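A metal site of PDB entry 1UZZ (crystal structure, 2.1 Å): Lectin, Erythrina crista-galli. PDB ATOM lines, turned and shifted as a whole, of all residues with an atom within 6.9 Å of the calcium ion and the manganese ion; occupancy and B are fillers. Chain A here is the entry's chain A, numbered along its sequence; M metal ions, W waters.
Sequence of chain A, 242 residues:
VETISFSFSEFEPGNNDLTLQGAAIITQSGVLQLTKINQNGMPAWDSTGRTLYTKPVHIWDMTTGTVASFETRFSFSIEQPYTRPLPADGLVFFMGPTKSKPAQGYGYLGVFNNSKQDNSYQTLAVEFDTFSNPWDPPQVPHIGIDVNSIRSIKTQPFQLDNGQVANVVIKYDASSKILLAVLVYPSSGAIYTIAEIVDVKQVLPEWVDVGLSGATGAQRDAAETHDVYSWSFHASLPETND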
ATOM      1  N   ASP A  89      18.015   6.113 -21.044  1.00  0.00           N
ATOM      2  CA  ASP A  89      17.846   5.926 -19.640  1.00  0.00           C
ATOM      3  C   ASP A  89      18.491   7.084 -18.889  1.00  0.00           C
ATOM      4  O   ASP A  89      18.140   7.546 -17.743  1.00  0.00           O
ATOM      5  CB  ASP A  89      18.462   4.524 -19.186  1.00  0.00           C
ATOM      6  CG  ASP A  89      17.505   3.441 -19.213  1.00  0.00           C
ATOM      7  OD1 ASP A  89      17.564   2.582 -20.205  1.00  0.00           O
ATOM      8  OD2 ASP A  89      16.795   3.180 -18.329  1.00  0.00           O
ATOM      9  N   GLY A  90      19.482   7.539 -19.505  1.00  0.00           N
ATOM     10  CA  GLY A  90      20.174   8.728 -18.828  1.00  0.00           C
ATOM     11  C   GLY A  90      21.687   8.730 -18.936  1.00  0.00           C
ATOM     12  O   GLY A  90      22.344   7.940 -19.786  1.00  0.00           O
ATOM     13  N   TYR A 106      21.306   0.119 -19.738  1.00  0.00           N
ATOM     14  CA  TYR A 106      19.916   0.418 -19.426  1.00  0.00           C
ATOM     15  C   TYR A 106      19.853   1.283 -18.168  1.00  0.00           C
ATOM     16  O   TYR A 106      20.683   2.157 -17.970  1.00  0.00           O
ATOM     17  CB  TYR A 106      19.126  -0.877 -19.187  1.00  0.00           C
ATOM     18  CG  TYR A 106      19.195  -1.856 -20.324  1.00  0.00           C
ATOM     19  CD1 TYR A 106      19.134  -3.228 -20.086  1.00  0.00           C
ATOM     20  CD2 TYR A 106      19.343  -1.421 -21.651  1.00  0.00           C
ATOM     21  CE1 TYR A 106      19.215  -4.142 -21.125  1.00  0.00           C
ATOM     22  CE2 TYR A 106      19.432  -2.329 -22.704  1.00  0.00           C
ATOM     23  CZ  TYR A 106      19.372  -3.691 -22.426  1.00  0.00           C
ATOM     24  OH  TYR A 106      19.459  -4.601 -23.446  1.00  0.00           O
ATOM     25  N   GLY A 107      18.861   1.007 -17.327  1.00  0.00           N
ATOM     26  CA  GLY A 107      18.706   1.768 -16.093  1.00  0.00           C
ATOM     27  C   GLY A 107      19.889   1.765 -15.144  1.00  0.00           C
ATOM     28  O   GLY A 107      19.914   2.548 -14.191  1.00  0.00           O
ATOM     29  N   TYR A 108      20.873   0.892 -15.377  1.00  0.00           N
ATOM     30  CA  TYR A 108      22.059   0.846 -14.515  1.00  0.00           C
ATOM     31  C   TYR A 108      23.100   1.846 -15.004  1.00  0.00           C
ATOM     32  O   TYR A 108      24.160   2.027 -14.382  1.00  0.00           O
ATOM     33  CB  TYR A 108      22.622  -0.569 -14.458  1.00  0.00           C
ATOM     34  CG  TYR A 108      21.628  -1.567 -13.908  1.00  0.00           C
ATOM     35  CD1 TYR A 108      20.995  -1.338 -12.690  1.00  0.00           C
ATOM     36  CD2 TYR A 108      21.283  -2.707 -14.633  1.00  0.00           C
ATOM     37  CE1 TYR A 108      20.017  -2.221 -12.214  1.00  0.00           C
ATOM     38  CE2 TYR A 108      20.313  -3.584 -14.171  1.00  0.00           C
ATOM     39  CZ  TYR A 108      19.681  -3.335 -12.958  1.00  0.00           C
ATOM     40  OH  TYR A 108      18.714  -4.200 -12.489  1.00  0.00           O
ATOM     41  N   LEU A 109      22.786   2.484 -16.127  1.00  0.00           N
ATOM     42  CA  LEU A 109      23.627   3.531 -16.729  1.00  0.00           C
ATOM     43  C   LEU A 109      25.101   3.199 -16.983  1.00  0.00           C
ATOM     44  O   LEU A 109      25.926   4.109 -17.059  1.00  0.00           O
ATOM     45  CB  LEU A 109      23.547   4.796 -15.857  1.00  0.00           C
ATOM     46  CG  LEU A 109      22.136   5.354 -15.631  1.00  0.00           C
ATOM     47  CD1 LEU A 109      22.188   6.507 -14.633  1.00  0.00           C
ATOM     48  CD2 LEU A 109      21.556   5.811 -16.966  1.00  0.00           C
ATOM     49  N   GLU A 127      23.760  11.204 -11.171  1.00  0.00           N
ATOM     50  CA  GLU A 127      23.037  10.838 -12.370  1.00  0.00           C
ATOM     51  C   GLU A 127      22.041  11.889 -12.794  1.00  0.00           C
ATOM     52  O   GLU A 127      21.645  12.739 -12.012  1.00  0.00           O
ATOM     53  CB  GLU A 127      22.269   9.533 -12.124  1.00  0.00           C
ATOM     54  CG  GLU A 127      21.312   9.651 -10.936  1.00  0.00           C
ATOM     55  CD  GLU A 127      20.395   8.472 -10.761  1.00  0.00           C
ATOM     56  OE1 GLU A 127      20.891   7.323 -10.650  1.00  0.00           O
ATOM     57  OE2 GLU A 127      19.172   8.683 -10.723  1.00  0.00           O
ATOM     58  N   PHE A 128      21.637  11.795 -14.063  1.00  0.00           N
ATOM     59  CA  PHE A 128      20.653  12.665 -14.672  1.00  0.00           C
ATOM     60  C   PHE A 128      19.833  11.610 -15.385  1.00  0.00           C
ATOM     61  O   PHE A 128      20.073  11.266 -16.538  1.00  0.00           O
ATOM     62  CB  PHE A 128      21.321  13.636 -15.623  1.00  0.00           C
ATOM     63  CG  PHE A 128      22.183  14.644 -14.921  1.00  0.00           C
ATOM     64  CD1 PHE A 128      21.622  15.818 -14.412  1.00  0.00           C
ATOM     65  CD2 PHE A 128      23.532  14.398 -14.700  1.00  0.00           C
ATOM     66  CE1 PHE A 128      22.391  16.721 -13.701  1.00  0.00           C
ATOM     67  CE2 PHE A 128      24.310  15.299 -13.992  1.00  0.00           C
ATOM     68  CZ  PHE A 128      23.736  16.463 -13.487  1.00  0.00           C
ATOM     69  N   ASP A 129      18.893  11.085 -14.619  1.00  0.00           N
ATOM     70  CA  ASP A 129      18.008   9.992 -14.964  1.00  0.00           C
ATOM     71  C   ASP A 129      16.746  10.341 -15.746  1.00  0.00           C
ATOM     72  O   ASP A 129      15.874  11.038 -15.238  1.00  0.00           O
ATOM     73  CB  ASP A 129      17.615   9.319 -13.661  1.00  0.00           C
ATOM     74  CG  ASP A 129      17.182   7.927 -13.843  1.00  0.00           C
ATOM     75  OD1 ASP A 129      16.669   7.613 -14.944  1.00  0.00           O
ATOM     76  OD2 ASP A 129      17.341   7.144 -12.887  1.00  0.00           O
ATOM     77  N   THR A 130      16.632   9.807 -16.965  1.00  0.00           N
ATOM     78  CA  THR A 130      15.485  10.087 -17.828  1.00  0.00           C
ATOM     79  C   THR A 130      14.333   9.074 -17.837  1.00  0.00           C
ATOM     80  O   THR A 130      13.260   9.357 -18.380  1.00  0.00           O
ATOM     81  CB  THR A 130      15.944  10.294 -19.288  1.00  0.00           C
ATOM     82  OG1 THR A 130      16.698   9.150 -19.711  1.00  0.00           O
ATOM     83  CG2 THR A 130      16.811  11.541 -19.411  1.00  0.00           C
ATOM     84  N   PHE A 131      14.538   7.891 -17.271  1.00  0.00           N
ATOM     85  CA  PHE A 131      13.494   6.856 -17.252  1.00  0.00           C
ATOM     86  C   PHE A 131      13.238   6.450 -15.795  1.00  0.00           C
ATOM     87  O   PHE A 131      14.146   6.395 -14.999  1.00  0.00           O
ATOM     88  CB  PHE A 131      13.938   5.634 -18.069  1.00  0.00           C
ATOM     89  CG  PHE A 131      12.906   4.526 -18.133  1.00  0.00           C
ATOM     90  CD1 PHE A 131      11.973   4.480 -19.175  1.00  0.00           C
ATOM     91  CD2 PHE A 131      12.863   3.531 -17.166  1.00  0.00           C
ATOM     92  CE1 PHE A 131      11.022   3.458 -19.250  1.00  0.00           C
ATOM     93  CE2 PHE A 131      11.914   2.501 -17.229  1.00  0.00           C
ATOM     94  CZ  PHE A 131      10.992   2.463 -18.276  1.00  0.00           C
ATOM     95  N   SER A 132      11.989   6.160 -15.451  1.00  0.00           N
ATOM     96  CA  SER A 132      11.671   5.786 -14.089  1.00  0.00           C
ATOM     97  C   SER A 132      11.575   4.267 -13.913  1.00  0.00           C
ATOM     98  O   SER A 132      10.566   3.658 -14.291  1.00  0.00           O
ATOM     99  CB  SER A 132      10.348   6.452 -13.658  1.00  0.00           C
ATOM    100  OG  SER A 132      10.057   6.202 -12.290  1.00  0.00           O
ATOM    101  N   ASN A 133      12.632   3.668 -13.356  1.00  0.00           N
ATOM    102  CA  ASN A 133      12.664   2.226 -13.086  1.00  0.00           C
ATOM    103  C   ASN A 133      11.960   1.974 -11.747  1.00  0.00           C
ATOM    104  O   ASN A 133      11.559   2.921 -11.071  1.00  0.00           O
ATOM    105  CB  ASN A 133      14.111   1.705 -12.990  1.00  0.00           C
ATOM    106  CG  ASN A 133      14.834   1.752 -14.318  1.00  0.00           C
ATOM    107  OD1 ASN A 133      15.387   2.770 -14.692  1.00  0.00           O
ATOM    108  ND2 ASN A 133      14.815   0.642 -15.048  1.00  0.00           N
ATOM    109  N   TRP A 135      13.105   1.201  -8.882  1.00  0.00           N
ATOM    110  CA  TRP A 135      13.837   1.750  -7.738  1.00  0.00           C
ATOM    111  C   TRP A 135      13.921   3.276  -7.763  1.00  0.00           C
ATOM    112  O   TRP A 135      14.538   3.879  -6.887  1.00  0.00           O
ATOM    113  CB  TRP A 135      15.250   1.173  -7.705  1.00  0.00           C
ATOM    114  CG  TRP A 135      16.049   1.566  -8.912  1.00  0.00           C
ATOM    115  CD1 TRP A 135      16.662   2.761  -9.141  1.00  0.00           C
ATOM    116  CD2 TRP A 135      16.265   0.773 -10.092  1.00  0.00           C
ATOM    117  NE1 TRP A 135      17.254   2.764 -10.390  1.00  0.00           N
ATOM    118  CE2 TRP A 135      17.027   1.564 -10.996  1.00  0.00           C
ATOM    119  CE3 TRP A 135      15.896  -0.527 -10.474  1.00  0.00           C
ATOM    120  CZ2 TRP A 135      17.422   1.092 -12.249  1.00  0.00           C
ATOM    121  CZ3 TRP A 135      16.282  -0.988 -11.727  1.00  0.00           C
ATOM    122  CH2 TRP A 135      17.043  -0.180 -12.603  1.00  0.00           C
ATOM    123  N   ASP A 136      13.316   3.903  -8.757  1.00  0.00           N
ATOM    124  CA  ASP A 136      13.357   5.359  -8.913  1.00  0.00           C
ATOM    125  C   ASP A 136      12.148   6.109  -8.405  1.00  0.00           C
ATOM    126  O   ASP A 136      11.080   5.538  -8.188  1.00  0.00           O
ATOM    127  CB  ASP A 136      13.463   5.742 -10.375  1.00  0.00           C
ATOM    128  CG  ASP A 136      14.836   5.568 -10.935  1.00  0.00           C
ATOM    129  OD1 ASP A 136      15.808   5.961 -10.272  1.00  0.00           O
ATOM    130  OD2 ASP A 136      14.916   5.037 -12.051  1.00  0.00           O
ATOM    131  N   PRO A 137      12.302   7.435  -8.223  1.00  0.00           N
ATOM    132  CA  PRO A 137      11.156   8.227  -7.776  1.00  0.00           C
ATOM    133  C   PRO A 137      10.335   8.266  -9.072  1.00  0.00           C
ATOM    134  O   PRO A 137      10.880   8.036 -10.147  1.00  0.00           O
ATOM    135  CB  PRO A 137      11.782   9.566  -7.424  1.00  0.00           C
ATOM    136  CG  PRO A 137      12.976   9.650  -8.321  1.00  0.00           C
ATOM    137  CD  PRO A 137      13.532   8.248  -8.255  1.00  0.00           C
ATOM    138  N   VAL A 140      10.631  11.974 -13.799  1.00  0.00           N
ATOM    139  CA  VAL A 140      11.816  11.969 -14.642  1.00  0.00           C
ATOM    140  C   VAL A 140      11.632  13.107 -15.630  1.00  0.00           C
ATOM    141  O   VAL A 140      10.520  13.403 -16.048  1.00  0.00           O
ATOM    142  CB  VAL A 140      11.997  10.648 -15.423  1.00  0.00           C
ATOM    143  CG1 VAL A 140      12.410   9.524 -14.484  1.00  0.00           C
ATOM    144  CG2 VAL A 140      10.700  10.290 -16.149  1.00  0.00           C
ATOM    145  N   HIS A 142      15.308  13.363 -13.468  1.00  0.00           N
ATOM    146  CA  HIS A 142      15.679  13.777 -12.125  1.00  0.00           C
ATOM    147  C   HIS A 142      17.172  13.659 -11.890  1.00  0.00           C
ATOM    148  O   HIS A 142      17.871  12.875 -12.540  1.00  0.00           O
ATOM    149  CB  HIS A 142      14.938  12.929 -11.075  1.00  0.00           C
ATOM    150  CG  HIS A 142      15.206  11.465 -11.166  1.00  0.00           C
ATOM    151  ND1 HIS A 142      14.370  10.588 -11.831  1.00  0.00           N
ATOM    152  CD2 HIS A 142      16.204  10.707 -10.640  1.00  0.00           C
ATOM    153  CE1 HIS A 142      14.836   9.359 -11.714  1.00  0.00           C
ATOM    154  NE2 HIS A 142      15.944   9.405 -11.000  1.00  0.00           N
ATOM    155  N   ILE A 143      17.670  14.476 -10.975  1.00  0.00           N
ATOM    156  CA  ILE A 143      19.075  14.431 -10.635  1.00  0.00           C
ATOM    157  C   ILE A 143      19.113  13.537  -9.406  1.00  0.00           C
ATOM    158  O   ILE A 143      18.136  13.476  -8.650  1.00  0.00           O
ATOM    159  CB  ILE A 143      19.627  15.818 -10.273  1.00  0.00           C
ATOM    160  CG1 ILE A 143      19.378  16.795 -11.429  1.00  0.00           C
ATOM    161  CG2 ILE A 143      21.107  15.717  -9.974  1.00  0.00           C
ATOM    162  CD1 ILE A 143      19.839  18.208 -11.152  1.00  0.00           C
ATOM    163  N   GLY A 144      20.220  12.844  -9.214  1.00  0.00           N
ATOM    164  CA  GLY A 144      20.325  11.978  -8.063  1.00  0.00           C
ATOM    165  C   GLY A 144      21.758  11.744  -7.603  1.00  0.00           C
ATOM    166  O   GLY A 144      22.686  11.690  -8.413  1.00  0.00           O
ATOM    167  N   ASP A 146      24.166   9.126  -6.064  1.00  0.00           N
ATOM    168  CA  ASP A 146      24.296   7.674  -5.894  1.00  0.00           C
ATOM    169  C   ASP A 146      25.525   7.270  -5.090  1.00  0.00           C
ATOM    170  O   ASP A 146      26.654   7.607  -5.441  1.00  0.00           O
ATOM    171  CB  ASP A 146      24.361   6.977  -7.266  1.00  0.00           C
ATOM    172  CG  ASP A 146      23.128   7.241  -8.133  1.00  0.00           C
ATOM    173  OD1 ASP A 146      22.018   7.348  -7.570  1.00  0.00           O
ATOM    174  OD2 ASP A 146      23.262   7.307  -9.370  1.00  0.00           O
ATOM    175  N   ILE A 150      22.414   2.304  -7.533  1.00  0.00           N
ATOM    176  CA  ILE A 150      21.676   3.041  -8.534  1.00  0.00           C
ATOM    177  C   ILE A 150      20.440   3.648  -7.858  1.00  0.00           C
ATOM    178  O   ILE A 150      19.751   4.486  -8.439  1.00  0.00           O
ATOM    179  CB  ILE A 150      21.225   2.110  -9.692  1.00  0.00           C
ATOM    180  CG1 ILE A 150      20.661   2.928 -10.859  1.00  0.00           C
ATOM    181  CG2 ILE A 150      20.186   1.112  -9.193  1.00  0.00           C
ATOM    182  CD1 ILE A 150      21.681   3.856 -11.518  1.00  0.00           C
ATOM    183  N   ARG A 151      20.174   3.208  -6.624  1.00  0.00           N
ATOM    184  CA  ARG A 151      19.035   3.721  -5.848  1.00  0.00           C
ATOM    185  C   ARG A 151      19.533   4.932  -5.088  1.00  0.00           C
ATOM    186  O   ARG A 151      19.999   4.822  -3.961  1.00  0.00           O
ATOM    187  CB  ARG A 151      18.538   2.671  -4.843  1.00  0.00           C
ATOM    188  CG  ARG A 151      17.941   1.395  -5.432  1.00  0.00           C
ATOM    189  CD  ARG A 151      17.543   0.453  -4.299  1.00  0.00           C
ATOM    190  NE  ARG A 151      17.076  -0.863  -4.767  1.00  0.00           N
ATOM    191  CZ  ARG A 151      15.822  -1.152  -5.084  1.00  0.00           C
ATOM    192  NH1 ARG A 151      14.881  -0.234  -4.991  1.00  0.00           N
ATOM    193  NH2 ARG A 151      15.508  -2.379  -5.488  1.00  0.00           N
ATOM    194  N   SER A 152      19.433   6.092  -5.721  1.00  0.00           N
ATOM    195  CA  SER A 152      19.888   7.361  -5.154  1.00  0.00           C
ATOM    196  C   SER A 152      19.507   7.585  -3.688  1.00  0.00           C
ATOM    197  O   SER A 152      18.405   7.223  -3.264  1.00  0.00           O
ATOM    198  CB  SER A 152      19.350   8.518  -5.991  1.00  0.00           C
ATOM    199  OG  SER A 152      19.453   8.220  -7.370  1.00  0.00           O
ATOM    200  N   THR A 155      17.195  12.532  -4.556  1.00  0.00           N
ATOM    201  CA  THR A 155      16.857  12.895  -5.917  1.00  0.00           C
ATOM    202  C   THR A 155      16.232  14.278  -6.035  1.00  0.00           C
ATOM    203  O   THR A 155      15.699  14.812  -5.065  1.00  0.00           O
ATOM    204  CB  THR A 155      15.871  11.886  -6.530  1.00  0.00           C
ATOM    205  OG1 THR A 155      14.746  11.740  -5.659  1.00  0.00           O
ATOM    206  CG2 THR A 155      16.554  10.545  -6.727  1.00  0.00           C
HETATM  207 CA    CA M   1      16.282   5.144 -14.220  1.00  0.00          CA
HETATM  208 MN    MN M   2      17.318   7.456 -10.767  1.00  0.00          MN
HETATM  209  O   HOH W   1      18.439   4.282 -12.907  1.00  0.00           O
HETATM  210  O   HOH W   2      18.761   5.639 -10.530  1.00  0.00           O
HETATM  211  O   HOH W   3      17.346   7.949  -8.617  1.00  0.00           O
HETATM  212  O   HOH W   4      17.006   4.753 -16.727  1.00  0.00           O
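OE2 of Glu 127 lies close to OG of Ser 152.
The side-chain carboxylate (OE1) of Glu 127 sits close to the side-chain carboxylate (OD2) of Asp 146, at 2.7 Å.
N of Glu 127 sits at hydrogen-bond distance from O of Gly 144, 3.0 Å away.
Along chain A the residues within 4 Å of the calcium ion span positions 129 to 136.
The nearest printed residue that does not touch the calcium ion is Gly 107 (4.5 Å).
Of the 25 residues printed, 4 come within 4 Å of the manganese ion.
The calcium ion is bound by the side-chain carboxylate (OD2) of Asp 136, the side-chain amide oxygen (OD1) of Asn 133, the backbone carbonyl oxygen (O) of Phe 131, the side-chain carboxylate (OD1) of Asp 129, the side-chain carboxylate (OD2) of Asp 129, water W4 and water W1.
The manganese ion is bound by OD2 of Asp 129 (2.1 Å), OD1 of Asp 136 (2.2 Å), water W3 (2.2 Å), OE2 of Glu 127 (2.2 Å), water W2 (2.3 Å) and NE2 of His 142 (2.4 Å).
Water W1 bridges O of Gly 107 and NE1 of Trp 135.
Water W2 lies within hydrogen-bond range of the backbone carbonyl oxygen (O) of Ile 150 (2.6 Å), the side-chain carboxylate (OE1) of Glu 127 (2.7 Å) and the indole nitrogen (NE1) of Trp 135 (3.2 Å).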
